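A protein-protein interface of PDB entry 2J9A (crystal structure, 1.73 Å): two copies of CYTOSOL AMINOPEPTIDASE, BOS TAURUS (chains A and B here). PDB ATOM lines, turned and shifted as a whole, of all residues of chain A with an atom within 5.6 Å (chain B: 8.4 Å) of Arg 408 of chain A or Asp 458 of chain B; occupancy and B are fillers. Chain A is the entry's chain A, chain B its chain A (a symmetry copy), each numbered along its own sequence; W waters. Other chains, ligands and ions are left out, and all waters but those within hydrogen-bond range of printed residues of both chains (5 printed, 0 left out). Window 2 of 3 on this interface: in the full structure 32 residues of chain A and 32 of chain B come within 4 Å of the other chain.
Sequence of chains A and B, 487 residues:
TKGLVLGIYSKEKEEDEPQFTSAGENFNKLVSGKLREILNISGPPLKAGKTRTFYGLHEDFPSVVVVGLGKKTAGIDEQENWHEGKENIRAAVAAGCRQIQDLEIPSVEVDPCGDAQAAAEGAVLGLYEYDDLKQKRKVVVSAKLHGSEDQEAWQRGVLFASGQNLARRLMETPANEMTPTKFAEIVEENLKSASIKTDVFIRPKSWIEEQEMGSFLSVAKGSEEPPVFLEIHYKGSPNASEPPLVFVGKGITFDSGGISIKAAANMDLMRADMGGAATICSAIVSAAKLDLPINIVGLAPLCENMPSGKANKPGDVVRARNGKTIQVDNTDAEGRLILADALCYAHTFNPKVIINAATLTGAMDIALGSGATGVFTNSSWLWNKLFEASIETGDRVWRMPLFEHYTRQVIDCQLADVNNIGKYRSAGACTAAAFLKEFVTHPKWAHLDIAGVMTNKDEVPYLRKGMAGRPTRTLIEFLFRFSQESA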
ATOM      1  N   GLU A 404     -13.881  -5.078 -31.073  1.00  0.00           N
ATOM      2  CA  GLU A 404     -14.138  -4.567 -29.730  1.00  0.00           C
ATOM      3  C   GLU A 404     -15.564  -4.934 -29.289  1.00  0.00           C
ATOM      4  O   GLU A 404     -15.828  -5.078 -28.097  1.00  0.00           O
ATOM      5  CB  GLU A 404     -13.873  -3.041 -29.660  1.00  0.00           C
ATOM      6  CG  GLU A 404     -14.165  -2.423 -28.290  1.00  0.00           C
ATOM      7  CD  GLU A 404     -15.646  -2.091 -28.035  1.00  0.00           C
ATOM      8  OE1 GLU A 404     -16.460  -2.034 -29.002  1.00  0.00           O
ATOM      9  OE2 GLU A 404     -15.985  -1.851 -26.834  1.00  0.00           O
ATOM     10  N   HIS A 405     -16.456  -5.174 -30.261  1.00  0.00           N
ATOM     11  CA  HIS A 405     -17.834  -5.656 -29.968  1.00  0.00           C
ATOM     12  C   HIS A 405     -17.785  -6.835 -28.952  1.00  0.00           C
ATOM     13  O   HIS A 405     -18.544  -6.877 -27.973  1.00  0.00           O
ATOM     14  CB  HIS A 405     -18.447  -6.083 -31.300  1.00  0.00           C
ATOM     15  CG  HIS A 405     -19.769  -6.810 -31.201  1.00  0.00           C
ATOM     16  ND1 HIS A 405     -20.931  -6.326 -31.775  1.00  0.00           N
ATOM     17  CD2 HIS A 405     -20.082  -8.027 -30.688  1.00  0.00           C
ATOM     18  CE1 HIS A 405     -21.908  -7.210 -31.604  1.00  0.00           C
ATOM     19  NE2 HIS A 405     -21.420  -8.250 -30.944  1.00  0.00           N
ATOM     20  N   TYR A 406     -16.864  -7.784 -29.197  1.00  0.00           N
ATOM     21  CA  TYR A 406     -16.751  -8.940 -28.289  1.00  0.00           C
ATOM     22  C   TYR A 406     -16.000  -8.567 -27.009  1.00  0.00           C
ATOM     23  O   TYR A 406     -16.341  -9.042 -25.914  1.00  0.00           O
ATOM     24  CB  TYR A 406     -16.050 -10.075 -29.047  1.00  0.00           C
ATOM     25  CG  TYR A 406     -16.747 -10.431 -30.368  1.00  0.00           C
ATOM     26  CD1 TYR A 406     -18.035 -11.048 -30.363  1.00  0.00           C
ATOM     27  CD2 TYR A 406     -16.141 -10.168 -31.599  1.00  0.00           C
ATOM     28  CE1 TYR A 406     -18.684 -11.387 -31.546  1.00  0.00           C
ATOM     29  CE2 TYR A 406     -16.779 -10.507 -32.831  1.00  0.00           C
ATOM     30  CZ  TYR A 406     -18.071 -11.117 -32.776  1.00  0.00           C
ATOM     31  OH  TYR A 406     -18.692 -11.436 -33.974  1.00  0.00           O
ATOM     32  N   THR A 407     -14.972  -7.732 -27.133  1.00  0.00           N
ATOM     33  CA  THR A 407     -14.246  -7.264 -25.937  1.00  0.00           C
ATOM     34  C   THR A 407     -15.193  -6.669 -24.898  1.00  0.00           C
ATOM     35  O   THR A 407     -15.071  -6.940 -23.707  1.00  0.00           O
ATOM     36  CB  THR A 407     -13.159  -6.224 -26.327  1.00  0.00           C
ATOM     37  OG1 THR A 407     -12.270  -6.836 -27.262  1.00  0.00           O
ATOM     38  CG2 THR A 407     -12.354  -5.754 -25.104  1.00  0.00           C
ATOM     39  N   ARG A 408     -16.154  -5.871 -25.353  1.00  0.00           N
ATOM     40  CA  ARG A 408     -17.050  -5.172 -24.448  1.00  0.00           C
ATOM     41  C   ARG A 408     -17.850  -6.166 -23.591  1.00  0.00           C
ATOM     42  O   ARG A 408     -18.230  -5.864 -22.464  1.00  0.00           O
ATOM     43  CB  ARG A 408     -17.961  -4.241 -25.258  1.00  0.00           C
ATOM     44  CG  ARG A 408     -18.688  -3.176 -24.445  1.00  0.00           C
ATOM     45  CD  ARG A 408     -19.694  -2.472 -25.356  1.00  0.00           C
ATOM     46  NE  ARG A 408     -20.735  -1.744 -24.627  1.00  0.00           N
ATOM     47  CZ  ARG A 408     -21.980  -1.589 -25.077  1.00  0.00           C
ATOM     48  NH1 ARG A 408     -22.332  -2.099 -26.244  1.00  0.00           N
ATOM     49  NH2 ARG A 408     -22.862  -0.907 -24.376  1.00  0.00           N
ATOM     50  N   GLN A 409     -18.066  -7.367 -24.113  1.00  0.00           N
ATOM     51  CA  GLN A 409     -18.820  -8.365 -23.398  1.00  0.00           C
ATOM     52  C   GLN A 409     -18.003  -9.135 -22.364  1.00  0.00           C
ATOM     53  O   GLN A 409     -18.578  -9.883 -21.566  1.00  0.00           O
ATOM     54  CB  GLN A 409     -19.504  -9.314 -24.395  1.00  0.00           C
ATOM     55  CG  GLN A 409     -20.495  -8.568 -25.286  1.00  0.00           C
ATOM     56  CD  GLN A 409     -21.174  -9.458 -26.264  1.00  0.00           C
ATOM     57  OE1 GLN A 409     -21.086 -10.687 -26.184  1.00  0.00           O
ATOM     58  NE2 GLN A 409     -21.861  -8.842 -27.232  1.00  0.00           N
ATOM     59  N   VAL A 410     -16.682  -8.978 -22.378  1.00  0.00           N
ATOM     60  CA  VAL A 410     -15.881  -9.605 -21.331  1.00  0.00           C
ATOM     61  C   VAL A 410     -15.319  -8.611 -20.319  1.00  0.00           C
ATOM     62  O   VAL A 410     -15.015  -8.990 -19.211  1.00  0.00           O
ATOM     63  CB  VAL A 410     -14.792 -10.528 -21.872  1.00  0.00           C
ATOM     64  CG1 VAL A 410     -15.398 -11.559 -22.819  1.00  0.00           C
ATOM     65  CG2 VAL A 410     -13.714  -9.771 -22.601  1.00  0.00           C
ATOM     66  N   ILE A 411     -15.146  -7.355 -20.720  1.00  0.00           N
ATOM     67  CA  ILE A 411     -14.707  -6.373 -19.726  1.00  0.00           C
ATOM     68  C   ILE A 411     -15.904  -5.798 -18.943  1.00  0.00           C
ATOM     69  O   ILE A 411     -15.706  -5.165 -17.933  1.00  0.00           O
ATOM     70  CB  ILE A 411     -13.718  -5.284 -20.292  1.00  0.00           C
ATOM     71  CG1 ILE A 411     -14.422  -4.323 -21.271  1.00  0.00           C
ATOM     72  CG2 ILE A 411     -12.489  -5.959 -20.900  1.00  0.00           C
ATOM     73  CD1 ILE A 411     -13.514  -3.100 -21.697  1.00  0.00           C
ATOM     74  N   ASP A 412     -17.124  -6.068 -19.395  1.00  0.00           N
ATOM     75  CA  ASP A 412     -18.322  -5.790 -18.582  1.00  0.00           C
ATOM     76  C   ASP A 412     -18.295  -6.831 -17.470  1.00  0.00           C
ATOM     77  O   ASP A 412     -18.603  -7.998 -17.707  1.00  0.00           O
ATOM     78  CB  ASP A 412     -19.591  -5.995 -19.418  1.00  0.00           C
ATOM     79  CG  ASP A 412     -20.852  -5.693 -18.619  1.00  0.00           C
ATOM     80  OD1 ASP A 412     -20.749  -4.913 -17.648  1.00  0.00           O
ATOM     81  OD2 ASP A 412     -21.925  -6.215 -18.967  1.00  0.00           O
ATOM     82  N   LYS A 423     -21.047 -12.112 -21.303  1.00  0.00           N
ATOM     83  CA  LYS A 423     -22.363 -11.845 -20.750  1.00  0.00           C
ATOM     84  C   LYS A 423     -23.485 -12.656 -21.443  1.00  0.00           C
ATOM     85  O   LYS A 423     -24.513 -12.903 -20.823  1.00  0.00           O
ATOM     86  CB  LYS A 423     -22.681 -10.333 -20.646  1.00  0.00           C
ATOM     87  CG  LYS A 423     -22.098  -9.407 -21.698  1.00  0.00           C
ATOM     88  CD  LYS A 423     -22.748  -8.000 -21.564  1.00  0.00           C
ATOM     89  CE  LYS A 423     -21.779  -6.835 -21.857  1.00  0.00           C
ATOM     90  NZ  LYS A 423     -21.856  -6.014 -23.159  1.00  0.00           N
ATOM     91  N   TYR A 424     -23.263 -13.108 -22.691  1.00  0.00           N
ATOM     92  CA  TYR A 424     -24.272 -13.850 -23.483  1.00  0.00           C
ATOM     93  C   TYR A 424     -23.731 -15.186 -24.052  1.00  0.00           C
ATOM     94  O   TYR A 424     -22.527 -15.375 -24.101  1.00  0.00           O
ATOM     95  CB  TYR A 424     -24.761 -12.963 -24.639  1.00  0.00           C
ATOM     96  CG  TYR A 424     -25.072 -11.494 -24.326  1.00  0.00           C
ATOM     97  CD1 TYR A 424     -26.086 -11.120 -23.414  1.00  0.00           C
ATOM     98  CD2 TYR A 424     -24.413 -10.485 -25.008  1.00  0.00           C
ATOM     99  CE1 TYR A 424     -26.380  -9.743 -23.158  1.00  0.00           C
ATOM    100  CE2 TYR A 424     -24.704  -9.115 -24.786  1.00  0.00           C
ATOM    101  CZ  TYR A 424     -25.680  -8.753 -23.849  1.00  0.00           C
ATOM    102  OH  TYR A 424     -25.927  -7.392 -23.646  1.00  0.00           O
ATOM    103  N   SER B 370     -23.821 -11.127 -32.842  1.00  0.00           N
ATOM    104  CA  SER B 370     -24.331  -9.992 -33.587  1.00  0.00           C
ATOM    105  C   SER B 370     -23.174  -9.154 -34.109  1.00  0.00           C
ATOM    106  O   SER B 370     -23.367  -8.014 -34.567  1.00  0.00           O
ATOM    107  CB  SER B 370     -25.201  -9.124 -32.635  1.00  0.00           C
ATOM    108  OG  SER B 370     -24.486  -8.723 -31.488  1.00  0.00           O
ATOM    109  N   THR B 455     -31.439  -9.510 -33.759  1.00  0.00           N
ATOM    110  CA  THR B 455     -31.827  -8.596 -32.668  1.00  0.00           C
ATOM    111  C   THR B 455     -30.653  -7.704 -32.255  1.00  0.00           C
ATOM    112  O   THR B 455     -29.471  -7.996 -32.580  1.00  0.00           O
ATOM    113  CB  THR B 455     -32.289  -9.368 -31.399  1.00  0.00           C
ATOM    114  OG1 THR B 455     -31.141 -10.029 -30.827  1.00  0.00           O
ATOM    115  CG2 THR B 455     -33.334 -10.412 -31.737  1.00  0.00           C
ATOM    116  N   ASN B 456     -30.992  -6.593 -31.609  1.00  0.00           N
ATOM    117  CA  ASN B 456     -30.010  -5.784 -30.886  1.00  0.00           C
ATOM    118  C   ASN B 456     -30.447  -5.652 -29.432  1.00  0.00           C
ATOM    119  O   ASN B 456     -31.650  -5.544 -29.127  1.00  0.00           O
ATOM    120  CB  ASN B 456     -29.931  -4.361 -31.486  1.00  0.00           C
ATOM    121  CG  ASN B 456     -28.659  -3.615 -31.073  1.00  0.00           C
ATOM    122  OD1 ASN B 456     -27.594  -4.091 -31.365  1.00  0.00           O
ATOM    123  ND2 ASN B 456     -28.771  -2.422 -30.425  1.00  0.00           N
ATOM    124  N   LYS B 457     -29.464  -5.725 -28.536  1.00  0.00           N
ATOM    125  CA  LYS B 457     -29.659  -5.379 -27.149  1.00  0.00           C
ATOM    126  C   LYS B 457     -29.063  -3.988 -27.030  1.00  0.00           C
ATOM    127  O   LYS B 457     -29.802  -3.008 -27.080  1.00  0.00           O
ATOM    128  CB  LYS B 457     -28.964  -6.414 -26.270  1.00  0.00           C
ATOM    129  CG  LYS B 457     -29.693  -7.768 -26.343  1.00  0.00           C
ATOM    130  CD  LYS B 457     -28.991  -8.846 -25.471  1.00  0.00           C
ATOM    131  CE  LYS B 457     -27.980  -9.659 -26.281  1.00  0.00           C
ATOM    132  NZ  LYS B 457     -28.673 -10.547 -27.266  1.00  0.00           N
ATOM    133  N   ASP B 458     -27.737  -3.920 -26.925  1.00  0.00           N
ATOM    134  CA  ASP B 458     -27.000  -2.664 -26.912  1.00  0.00           C
ATOM    135  C   ASP B 458     -25.758  -2.677 -27.778  1.00  0.00           C
ATOM    136  O   ASP B 458     -24.926  -1.743 -27.678  1.00  0.00           O
ATOM    137  CB  ASP B 458     -26.514  -2.382 -25.471  1.00  0.00           C
ATOM    138  CG  ASP B 458     -25.617  -3.479 -24.904  1.00  0.00           C
ATOM    139  OD1 ASP B 458     -25.386  -4.612 -25.471  1.00  0.00           O
ATOM    140  OD2 ASP B 458     -25.147  -3.241 -23.780  1.00  0.00           O
ATOM    141  N   GLU B 459     -25.598  -3.701 -28.612  1.00  0.00           N
ATOM    142  CA  GLU B 459     -24.288  -3.885 -29.249  1.00  0.00           C
ATOM    143  C   GLU B 459     -24.020  -2.820 -30.284  1.00  0.00           C
ATOM    144  O   GLU B 459     -22.873  -2.273 -30.353  1.00  0.00           O
ATOM    145  CB  GLU B 459     -24.188  -5.245 -29.931  1.00  0.00           C
ATOM    146  CG  GLU B 459     -24.425  -6.419 -28.949  1.00  0.00           C
ATOM    147  CD  GLU B 459     -25.834  -6.916 -29.046  1.00  0.00           C
ATOM    148  OE1 GLU B 459     -26.761  -6.109 -28.814  1.00  0.00           O
ATOM    149  OE2 GLU B 459     -26.026  -8.114 -29.385  1.00  0.00           O
ATOM    150  N   VAL B 460     -25.079  -2.551 -31.075  1.00  0.00           N
ATOM    151  CA  VAL B 460     -25.050  -1.440 -32.075  1.00  0.00           C
ATOM    152  C   VAL B 460     -25.658  -0.234 -31.331  1.00  0.00           C
ATOM    153  O   VAL B 460     -26.813  -0.269 -30.946  1.00  0.00           O
ATOM    154  CB  VAL B 460     -25.868  -1.788 -33.300  1.00  0.00           C
ATOM    155  CG1 VAL B 460     -25.849  -0.603 -34.266  1.00  0.00           C
ATOM    156  CG2 VAL B 460     -25.309  -3.060 -33.991  1.00  0.00           C
ATOM    157  N   PRO B 461     -24.860   0.802 -31.051  1.00  0.00           N
ATOM    158  CA  PRO B 461     -25.281   1.847 -30.106  1.00  0.00           C
ATOM    159  C   PRO B 461     -26.463   2.643 -30.640  1.00  0.00           C
ATOM    160  O   PRO B 461     -27.266   3.149 -29.858  1.00  0.00           O
ATOM    161  CB  PRO B 461     -24.054   2.754 -29.995  1.00  0.00           C
ATOM    162  CG  PRO B 461     -22.894   1.921 -30.472  1.00  0.00           C
ATOM    163  CD  PRO B 461     -23.503   1.028 -31.556  1.00  0.00           C
ATOM    164  N   TYR B 462     -26.587   2.715 -31.950  1.00  0.00           N
ATOM    165  CA  TYR B 462     -27.670   3.515 -32.568  1.00  0.00           C
ATOM    166  C   TYR B 462     -28.933   2.725 -32.909  1.00  0.00           C
ATOM    167  O   TYR B 462     -29.775   3.209 -33.670  1.00  0.00           O
ATOM    168  CB  TYR B 462     -27.169   4.231 -33.833  1.00  0.00           C
ATOM    169  CG  TYR B 462     -26.345   3.401 -34.803  1.00  0.00           C
ATOM    170  CD1 TYR B 462     -24.941   3.294 -34.659  1.00  0.00           C
ATOM    171  CD2 TYR B 462     -26.964   2.719 -35.857  1.00  0.00           C
ATOM    172  CE1 TYR B 462     -24.182   2.540 -35.578  1.00  0.00           C
ATOM    173  CE2 TYR B 462     -26.217   1.965 -36.779  1.00  0.00           C
ATOM    174  CZ  TYR B 462     -24.828   1.873 -36.607  1.00  0.00           C
ATOM    175  OH  TYR B 462     -24.124   1.144 -37.517  1.00  0.00           O
ATOM    176  N   LEU B 463     -29.063   1.488 -32.411  1.00  0.00           N
ATOM    177  CA  LEU B 463     -30.327   0.771 -32.531  1.00  0.00           C
ATOM    178  C   LEU B 463     -30.877   0.514 -31.127  1.00  0.00           C
ATOM    179  O   LEU B 463     -30.164  -0.029 -30.271  1.00  0.00           O
ATOM    180  CB  LEU B 463     -30.129  -0.568 -33.259  1.00  0.00           C
ATOM    181  CG  LEU B 463     -29.532  -0.468 -34.659  1.00  0.00           C
ATOM    182  CD1 LEU B 463     -29.245  -1.905 -35.156  1.00  0.00           C
ATOM    183  CD2 LEU B 463     -30.496   0.252 -35.614  1.00  0.00           C
ATOM    184  N   ARG B 464     -32.105   0.948 -30.852  1.00  0.00           N
ATOM    185  CA  ARG B 464     -32.712   0.561 -29.574  1.00  0.00           C
ATOM    186  C   ARG B 464     -32.925  -0.973 -29.515  1.00  0.00           C
ATOM    187  O   ARG B 464     -32.855  -1.663 -30.559  1.00  0.00           O
ATOM    188  CB  ARG B 464     -34.025   1.314 -29.422  1.00  0.00           C
ATOM    189  CG  ARG B 464     -33.711   2.792 -29.148  1.00  0.00           C
ATOM    190  CD  ARG B 464     -34.990   3.643 -29.173  1.00  0.00           C
ATOM    191  NE  ARG B 464     -34.911   4.725 -28.192  1.00  0.00           N
ATOM    192  CZ  ARG B 464     -35.580   5.876 -28.289  1.00  0.00           C
ATOM    193  NH1 ARG B 464     -36.312   6.095 -29.362  1.00  0.00           N
ATOM    194  NH2 ARG B 464     -35.477   6.817 -27.334  1.00  0.00           N
ATOM    195  N   LYS B 465     -33.194  -1.487 -28.317  1.00  0.00           N
ATOM    196  CA  LYS B 465     -33.440  -2.917 -28.152  1.00  0.00           C
ATOM    197  C   LYS B 465     -34.583  -3.376 -29.062  1.00  0.00           C
ATOM    198  O   LYS B 465     -35.606  -2.706 -29.170  1.00  0.00           O
ATOM    199  CB  LYS B 465     -33.760  -3.244 -26.692  1.00  0.00           C
ATOM    200  CG  LYS B 465     -34.002  -4.713 -26.445  1.00  0.00           C
ATOM    201  CD  LYS B 465     -34.516  -5.015 -25.045  1.00  0.00           C
ATOM    202  CE  LYS B 465     -34.420  -6.493 -24.733  1.00  0.00           C
ATOM    203  NZ  LYS B 465     -35.200  -6.818 -23.500  1.00  0.00           N
ATOM    204  N   GLY B 466     -34.374  -4.485 -29.756  1.00  0.00           N
ATOM    205  CA  GLY B 466     -35.447  -5.078 -30.564  1.00  0.00           C
ATOM    206  C   GLY B 466     -34.889  -5.588 -31.875  1.00  0.00           C
ATOM    207  O   GLY B 466     -33.663  -5.779 -31.993  1.00  0.00           O
HETATM  208  O   HOH W   1     -22.546  -5.751 -25.586  1.00  0.00           O
HETATM  209  O   HOH W   2     -24.644 -10.076 -28.398  1.00  0.00           O
HETATM  210  O   HOH W   3     -24.569   0.750 -26.788  1.00  0.00           O
HETATM  211  O   HOH W   4     -20.945  -3.199 -28.841  1.00  0.00           O
HETATM  212  O   HOH W   5     -22.566 -10.837 -30.142  1.00  0.00           O
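CE1 of His 405 of chain A touches CB of Glu 459 of chain B, at 3.4 Å. Glu 459 of chain B touches Gln 409 of chain A. CZ of Tyr 424 of chain A touches CE of Lys 457 of chain B (3.5 Å).
Water W1 lies within hydrogen-bond range of NZ of Lys 423 of chain A (2.5 Å) and OD1 of Asp 458 of chain B (3.1 Å). Water W2 lies within hydrogen-bond range of the side-chain carboxylate (OE2) of Glu 459 of chain B (2.6 Å), the side-chain amide nitrogen (NE2) of Gln 409 of chain A (3.3 Å) and the side-chain hydroxyl (OG) of Ser 370 of chain B (3.4 Å). Water W4 lies within hydrogen-bond range of O of Glu 459 of chain B (2.6 Å) and NH1 of Arg 408 of chain A (3.1 Å). Water W3 lies within hydrogen-bond range of the backbone carbonyl oxygen of Asp 458 of chain B and the guanidinium group of Arg 408 of chain A. Water W5 bridges NE2 of His 405 of chain A (2.9 Å) and N of Ser 370 of chain B (3.0 Å).
Of the 13 printed residues of chain B, 4 touch a printed residue of chain A. Printed residues of chain B that touch a printed residue of chain A: Ser 370, Lys 457, Asp 458 and Glu 459.
NE2 of His 405 of chain A sits close to OG of Ser 370 of chain B (3.1 Å). The side-chain carboxylate (OD2) of Asp 458 of chain B lies within salt-bridge range of the guanidinium group (NH2) of Arg 408 of chain A, at 3.3 Å. OD1 of Asp 458 of chain B lies within hydrogen-bond range of OH of Tyr 424 of chain A.
No position is printed for both chains. Of the 6 pairs that touch across the chains among the printed residues, none has its exchanged pair printed and touching as well.
N of Lys 423 of chain A is in hydrogen-bond range of O of Gln 409 of chain A, 3.3 Å away. The side-chain hydroxyl (OG) of Ser 370 of chain B lies within hydrogen-bond range of the side-chain carboxylate (OE2) of Glu 459 of chain B, at 2.7 Å. The side-chain carboxylate of Glu 459 of chain B lies close to the side-chain amide oxygen of Asn 456 of chain B (3.4 Å). N of Lys 457 of chain B is in hydrogen-bond range of OE1 of Glu 459 of chain B (2.7 Å).
Printed residues of chain B within 4 Å of His 405 of chain A: Ser 370 and Glu 459. Printed residues of chain B within 4 Å of Gln 409 of chain A: Glu 459. Printed residues of chain A within 4 Å of Ser 370 of chain B: His 405 (3.0 Å). Printed residues of chain A within 4 Å of Lys 457 of chain B: Tyr 424. Of the printed residues of chain A, Glu 459 of chain B touches His 405 (3.4 Å) and Gln 409 (3.9 Å). The nearest printed residue of chain B that does not touch Arg 408 of chain A is Glu 459 of chain B (4.01 Å). The nearest printed residue of chain A that does not touch Asp 458 of chain B is Lys 423 of chain A (4.3 Å).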
